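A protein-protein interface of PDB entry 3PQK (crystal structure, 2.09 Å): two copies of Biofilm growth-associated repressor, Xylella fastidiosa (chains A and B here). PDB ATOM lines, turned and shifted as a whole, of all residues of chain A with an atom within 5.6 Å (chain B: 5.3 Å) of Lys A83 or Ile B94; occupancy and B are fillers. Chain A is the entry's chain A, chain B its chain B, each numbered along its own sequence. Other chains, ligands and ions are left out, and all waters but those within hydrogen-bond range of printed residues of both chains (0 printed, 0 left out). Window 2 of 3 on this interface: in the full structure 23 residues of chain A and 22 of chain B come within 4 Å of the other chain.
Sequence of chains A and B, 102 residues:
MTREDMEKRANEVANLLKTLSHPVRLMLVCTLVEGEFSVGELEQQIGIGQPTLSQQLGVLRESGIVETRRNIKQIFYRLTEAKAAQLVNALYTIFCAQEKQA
The side-chain amino group (NZ) of Lys A83 is in hydrogen-bond range of the backbone carbonyl oxygen (O) of Ile B94 (2.6 Å).
OE1 of Gln A86 lies within hydrogen-bond range of NZ of Lys A83, at 2.8 Å. The backbone NH (N) of Cys B96 sits at hydrogen-bond distance from the backbone carbonyl oxygen (O) of Leu B91 (3.5 Å).
Arg A9 touches Phe B95. Lys A83 touches Phe B95 (CG to CE1, 3.9 Å). Gln A86 touches Ile B94 (OE1 to CG2, 3.4 Å). Leu A87 touches Leu B91 (CD1 to CD2, 3.8 Å). CA of Leu A87 touches CD1 of Ile B94 (3.8 Å). Ala A90 touches Ala B90. CB of Ala A90 touches CD1 of Ile B94, 3.996 Å away.
Of the printed residues of chain B, Arg A9 touches Phe B95 (3.6 Å). Lys A83 touches just these residues of chain B: Ile B94 (2.6 Å) and Phe B95 (3.9 Å). Printed residues of chain B within 4 Å of Gln A86: Ile B94 (3.4 Å). Of the printed residues of chain B, Leu A87 touches Leu B91 and Ile B94. Thr B93 touches none of the printed residues of chain A. Of the printed residues of chain A, Ile B94 touches Lys A83, Gln A86, Leu A87 and Ala A90. The nearest printed residue of chain A that does not touch Ile B94 is Arg A9 (5.6 Å).
Hydrophobic or aromatic side chains of chain B that line the printed part of chain A: Ala B90, Leu B91, Ile B94 and Phe B95. Of the 9 printed residues of chain A, 5 touch a printed residue of chain B. Hydrophobic or aromatic side chains of chain A within 4 Å of the printed part of chain B: Leu A87 and Ala A90. Among the printed residues, 8 pairs touch across the chains. Among the printed residues, no Asp or Glu carboxylate lies within 4 Å of a Lys or Arg side-chain nitrogen of the other chain.
Ala A90 touches its own counterpart, Ala B90. Position printed for both chains: 90.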
ATOM      1  N   ARG A   9      -7.726 -22.117 -34.718  1.00  0.00           N
ATOM      2  CA  ARG A   9      -8.446 -22.219 -33.446  1.00  0.00           C
ATOM      3  C   ARG A   9      -7.507 -22.453 -32.258  1.00  0.00           C
ATOM      4  O   ARG A   9      -7.670 -21.803 -31.231  1.00  0.00           O
ATOM      5  CB  ARG A   9      -9.504 -23.332 -33.498  1.00  0.00           C
ATOM      6  CG  ARG A   9     -10.704 -23.093 -32.571  1.00  0.00           C
ATOM      7  CD  ARG A   9     -11.872 -22.539 -33.382  1.00  0.00           C
ATOM      8  NE  ARG A   9     -12.790 -21.691 -32.613  1.00  0.00           N
ATOM      9  CZ  ARG A   9     -12.530 -20.447 -32.203  1.00  0.00           C
ATOM     10  NH1 ARG A   9     -11.337 -19.904 -32.415  1.00  0.00           N
ATOM     11  NH2 ARG A   9     -13.449 -19.755 -31.543  1.00  0.00           N
ATOM     12  N   GLU A  81     -20.875 -10.734 -24.101  1.00  0.00           N
ATOM     13  CA  GLU A  81     -21.709 -11.826 -24.596  1.00  0.00           C
ATOM     14  C   GLU A  81     -20.986 -12.595 -25.713  1.00  0.00           C
ATOM     15  O   GLU A  81     -21.565 -13.473 -26.366  1.00  0.00           O
ATOM     16  CB  GLU A  81     -23.077 -11.299 -25.045  1.00  0.00           C
ATOM     17  CG  GLU A  81     -23.989 -10.921 -23.890  1.00  0.00           C
ATOM     18  CD  GLU A  81     -25.389 -10.543 -24.326  1.00  0.00           C
ATOM     19  OE1 GLU A  81     -25.561  -9.427 -24.870  1.00  0.00           O
ATOM     20  OE2 GLU A  81     -26.313 -11.368 -24.138  1.00  0.00           O
ATOM     21  N   ALA A  82     -19.690 -12.305 -25.861  1.00  0.00           N
ATOM     22  CA  ALA A  82     -18.801 -12.914 -26.841  1.00  0.00           C
ATOM     23  C   ALA A  82     -18.505 -14.368 -26.509  1.00  0.00           C
ATOM     24  O   ALA A  82     -18.856 -14.866 -25.430  1.00  0.00           O
ATOM     25  CB  ALA A  82     -17.500 -12.122 -26.905  1.00  0.00           C
ATOM     26  N   LYS A  83     -17.841 -15.039 -27.452  1.00  0.00           N
ATOM     27  CA  LYS A  83     -17.415 -16.429 -27.395  1.00  0.00           C
ATOM     28  C   LYS A  83     -16.692 -16.794 -26.076  1.00  0.00           C
ATOM     29  O   LYS A  83     -16.979 -17.841 -25.522  1.00  0.00           O
ATOM     30  CB  LYS A  83     -16.555 -16.744 -28.647  1.00  0.00           C
ATOM     31  CG  LYS A  83     -16.122 -18.200 -28.795  1.00  0.00           C
ATOM     32  CD  LYS A  83     -17.288 -19.085 -29.166  1.00  0.00           C
ATOM     33  CE  LYS A  83     -16.815 -20.481 -29.424  1.00  0.00           C
ATOM     34  NZ  LYS A  83     -17.910 -21.444 -29.204  1.00  0.00           N
ATOM     35  N   ALA A  84     -15.785 -15.935 -25.581  1.00  0.00           N
ATOM     36  CA  ALA A  84     -15.032 -16.141 -24.338  1.00  0.00           C
ATOM     37  C   ALA A  84     -15.909 -16.329 -23.059  1.00  0.00           C
ATOM     38  O   ALA A  84     -15.469 -16.971 -22.095  1.00  0.00           O
ATOM     39  CB  ALA A  84     -14.073 -14.989 -24.130  1.00  0.00           C
ATOM     40  N   ALA A  85     -17.118 -15.745 -23.043  1.00  0.00           N
ATOM     41  CA  ALA A  85     -18.026 -15.851 -21.889  1.00  0.00           C
ATOM     42  C   ALA A  85     -18.475 -17.310 -21.693  1.00  0.00           C
ATOM     43  O   ALA A  85     -18.758 -17.716 -20.560  1.00  0.00           O
ATOM     44  CB  ALA A  85     -19.238 -14.946 -22.080  1.00  0.00           C
ATOM     45  N   GLN A  86     -18.466 -18.105 -22.792  1.00  0.00           N
ATOM     46  CA  GLN A  86     -18.812 -19.539 -22.769  1.00  0.00           C
ATOM     47  C   GLN A  86     -17.736 -20.285 -21.979  1.00  0.00           C
ATOM     48  O   GLN A  86     -18.046 -21.166 -21.191  1.00  0.00           O
ATOM     49  CB  GLN A  86     -18.911 -20.111 -24.209  1.00  0.00           C
ATOM     50  CG  GLN A  86     -20.114 -19.616 -25.062  1.00  0.00           C
ATOM     51  CD  GLN A  86     -20.029 -20.088 -26.528  1.00  0.00           C
ATOM     52  OE1 GLN A  86     -19.443 -21.128 -26.858  1.00  0.00           O
ATOM     53  NE2 GLN A  86     -20.596 -19.324 -27.463  1.00  0.00           N
ATOM     54  N   LEU A  87     -16.475 -19.895 -22.152  1.00  0.00           N
ATOM     55  CA  LEU A  87     -15.383 -20.543 -21.431  1.00  0.00           C
ATOM     56  C   LEU A  87     -15.455 -20.153 -19.944  1.00  0.00           C
ATOM     57  O   LEU A  87     -15.303 -21.023 -19.077  1.00  0.00           O
ATOM     58  CB  LEU A  87     -14.004 -20.184 -22.043  1.00  0.00           C
ATOM     59  CG  LEU A  87     -12.753 -20.719 -21.271  1.00  0.00           C
ATOM     60  CD1 LEU A  87     -12.779 -22.226 -21.114  1.00  0.00           C
ATOM     61  CD2 LEU A  87     -11.457 -20.257 -21.946  1.00  0.00           C
ATOM     62  N   ALA A  90     -18.022 -22.129 -18.197  1.00  0.00           N
ATOM     63  CA  ALA A  90     -17.556 -23.504 -17.970  1.00  0.00           C
ATOM     64  C   ALA A  90     -16.590 -23.574 -16.812  1.00  0.00           C
ATOM     65  O   ALA A  90     -16.665 -24.511 -16.032  1.00  0.00           O
ATOM     66  CB  ALA A  90     -16.899 -24.060 -19.220  1.00  0.00           C
ATOM     67  N   ASN B  89     -12.760 -31.415 -21.742  1.00  0.00           N
ATOM     68  CA  ASN B  89     -14.063 -31.718 -22.329  1.00  0.00           C
ATOM     69  C   ASN B  89     -14.874 -30.440 -22.663  1.00  0.00           C
ATOM     70  O   ASN B  89     -15.533 -30.407 -23.697  1.00  0.00           O
ATOM     71  CB  ASN B  89     -14.845 -32.665 -21.414  1.00  0.00           C
ATOM     72  CG  ASN B  89     -14.504 -34.124 -21.637  1.00  0.00           C
ATOM     73  OD1 ASN B  89     -14.098 -34.838 -20.722  1.00  0.00           O
ATOM     74  ND2 ASN B  89     -14.641 -34.602 -22.863  1.00  0.00           N
ATOM     75  N   ALA B  90     -14.776 -29.378 -21.824  1.00  0.00           N
ATOM     76  CA  ALA B  90     -15.459 -28.098 -22.057  1.00  0.00           C
ATOM     77  C   ALA B  90     -14.816 -27.334 -23.191  1.00  0.00           C
ATOM     78  O   ALA B  90     -15.529 -26.732 -23.982  1.00  0.00           O
ATOM     79  CB  ALA B  90     -15.449 -27.245 -20.796  1.00  0.00           C
ATOM     80  N   LEU B  91     -13.475 -27.334 -23.269  1.00  0.00           N
ATOM     81  CA  LEU B  91     -12.752 -26.667 -24.361  1.00  0.00           C
ATOM     82  C   LEU B  91     -13.100 -27.356 -25.698  1.00  0.00           C
ATOM     83  O   LEU B  91     -13.233 -26.675 -26.723  1.00  0.00           O
ATOM     84  CB  LEU B  91     -11.228 -26.730 -24.130  1.00  0.00           C
ATOM     85  CG  LEU B  91     -10.641 -25.910 -22.971  1.00  0.00           C
ATOM     86  CD1 LEU B  91      -9.230 -26.402 -22.624  1.00  0.00           C
ATOM     87  CD2 LEU B  91     -10.614 -24.386 -23.304  1.00  0.00           C
ATOM     88  N   TYR B  92     -13.272 -28.703 -25.682  1.00  0.00           N
ATOM     89  CA  TYR B  92     -13.642 -29.470 -26.888  1.00  0.00           C
ATOM     90  C   TYR B  92     -14.992 -28.989 -27.392  1.00  0.00           C
ATOM     91  O   TYR B  92     -15.069 -28.512 -28.533  1.00  0.00           O
ATOM     92  CB  TYR B  92     -13.675 -30.991 -26.629  1.00  0.00           C
ATOM     93  CG  TYR B  92     -14.049 -31.815 -27.850  1.00  0.00           C
ATOM     94  CD1 TYR B  92     -13.104 -32.118 -28.829  1.00  0.00           C
ATOM     95  CD2 TYR B  92     -15.332 -32.329 -28.003  1.00  0.00           C
ATOM     96  CE1 TYR B  92     -13.438 -32.873 -29.951  1.00  0.00           C
ATOM     97  CE2 TYR B  92     -15.676 -33.099 -29.117  1.00  0.00           C
ATOM     98  CZ  TYR B  92     -14.722 -33.371 -30.085  1.00  0.00           C
ATOM     99  OH  TYR B  92     -15.041 -34.124 -31.187  1.00  0.00           O
ATOM    100  N   THR B  93     -16.027 -29.039 -26.515  1.00  0.00           N
ATOM    101  CA  THR B  93     -17.414 -28.628 -26.815  1.00  0.00           C
ATOM    102  C   THR B  93     -17.517 -27.160 -27.282  1.00  0.00           C
ATOM    103  O   THR B  93     -18.240 -26.868 -28.236  1.00  0.00           O
ATOM    104  CB  THR B  93     -18.331 -28.880 -25.596  1.00  0.00           C
ATOM    105  OG1 THR B  93     -18.237 -30.249 -25.191  1.00  0.00           O
ATOM    106  CG2 THR B  93     -19.795 -28.543 -25.884  1.00  0.00           C
ATOM    107  N   ILE B  94     -16.819 -26.243 -26.604  1.00  0.00           N
ATOM    108  CA  ILE B  94     -16.896 -24.820 -26.958  1.00  0.00           C
ATOM    109  C   ILE B  94     -16.133 -24.508 -28.241  1.00  0.00           C
ATOM    110  O   ILE B  94     -16.645 -23.767 -29.077  1.00  0.00           O
ATOM    111  CB  ILE B  94     -16.428 -23.910 -25.782  1.00  0.00           C
ATOM    112  CG1 ILE B  94     -17.312 -24.086 -24.523  1.00  0.00           C
ATOM    113  CG2 ILE B  94     -16.380 -22.436 -26.208  1.00  0.00           C
ATOM    114  CD1 ILE B  94     -16.567 -23.737 -23.189  1.00  0.00           C
ATOM    115  N   PHE B  95     -14.896 -25.031 -28.380  1.00  0.00           N
ATOM    116  CA  PHE B  95     -14.031 -24.671 -29.499  1.00  0.00           C
ATOM    117  C   PHE B  95     -13.746 -25.729 -30.571  1.00  0.00           C
ATOM    118  O   PHE B  95     -14.023 -25.484 -31.747  1.00  0.00           O
ATOM    119  CB  PHE B  95     -12.698 -24.092 -28.971  1.00  0.00           C
ATOM    120  CG  PHE B  95     -12.835 -22.913 -28.037  1.00  0.00           C
ATOM    121  CD1 PHE B  95     -13.070 -21.629 -28.536  1.00  0.00           C
ATOM    122  CD2 PHE B  95     -12.701 -23.074 -26.657  1.00  0.00           C
ATOM    123  CE1 PHE B  95     -13.198 -20.535 -27.680  1.00  0.00           C
ATOM    124  CE2 PHE B  95     -12.801 -21.972 -25.798  1.00  0.00           C
ATOM    125  CZ  PHE B  95     -13.047 -20.707 -26.317  1.00  0.00           C
ATOM    126  N   CYS B  96     -13.104 -26.841 -30.188  1.00  0.00           N
ATOM    127  CA  CYS B  96     -12.656 -27.893 -31.101  1.00  0.00           C
ATOM    128  C   CYS B  96     -13.760 -28.556 -31.892  1.00  0.00           C
ATOM    129  O   CYS B  96     -13.562 -28.813 -33.083  1.00  0.00           O
ATOM    130  CB  CYS B  96     -11.781 -28.907 -30.371  1.00  0.00           C
ATOM    131  SG  CYS B  96     -10.498 -28.137 -29.339  1.00  0.00           S
ATOM    132  N   GLN B  98     -16.362 -27.245 -33.132  1.00  0.00           N
ATOM    133  CA  GLN B  98     -16.840 -26.334 -34.187  1.00  0.00           C
ATOM    134  C   GLN B  98     -16.140 -26.556 -35.546  1.00  0.00           C
ATOM    135  O   GLN B  98     -16.604 -26.042 -36.570  1.00  0.00           O
ATOM    136  CB  GLN B  98     -16.698 -24.859 -33.747  1.00  0.00           C
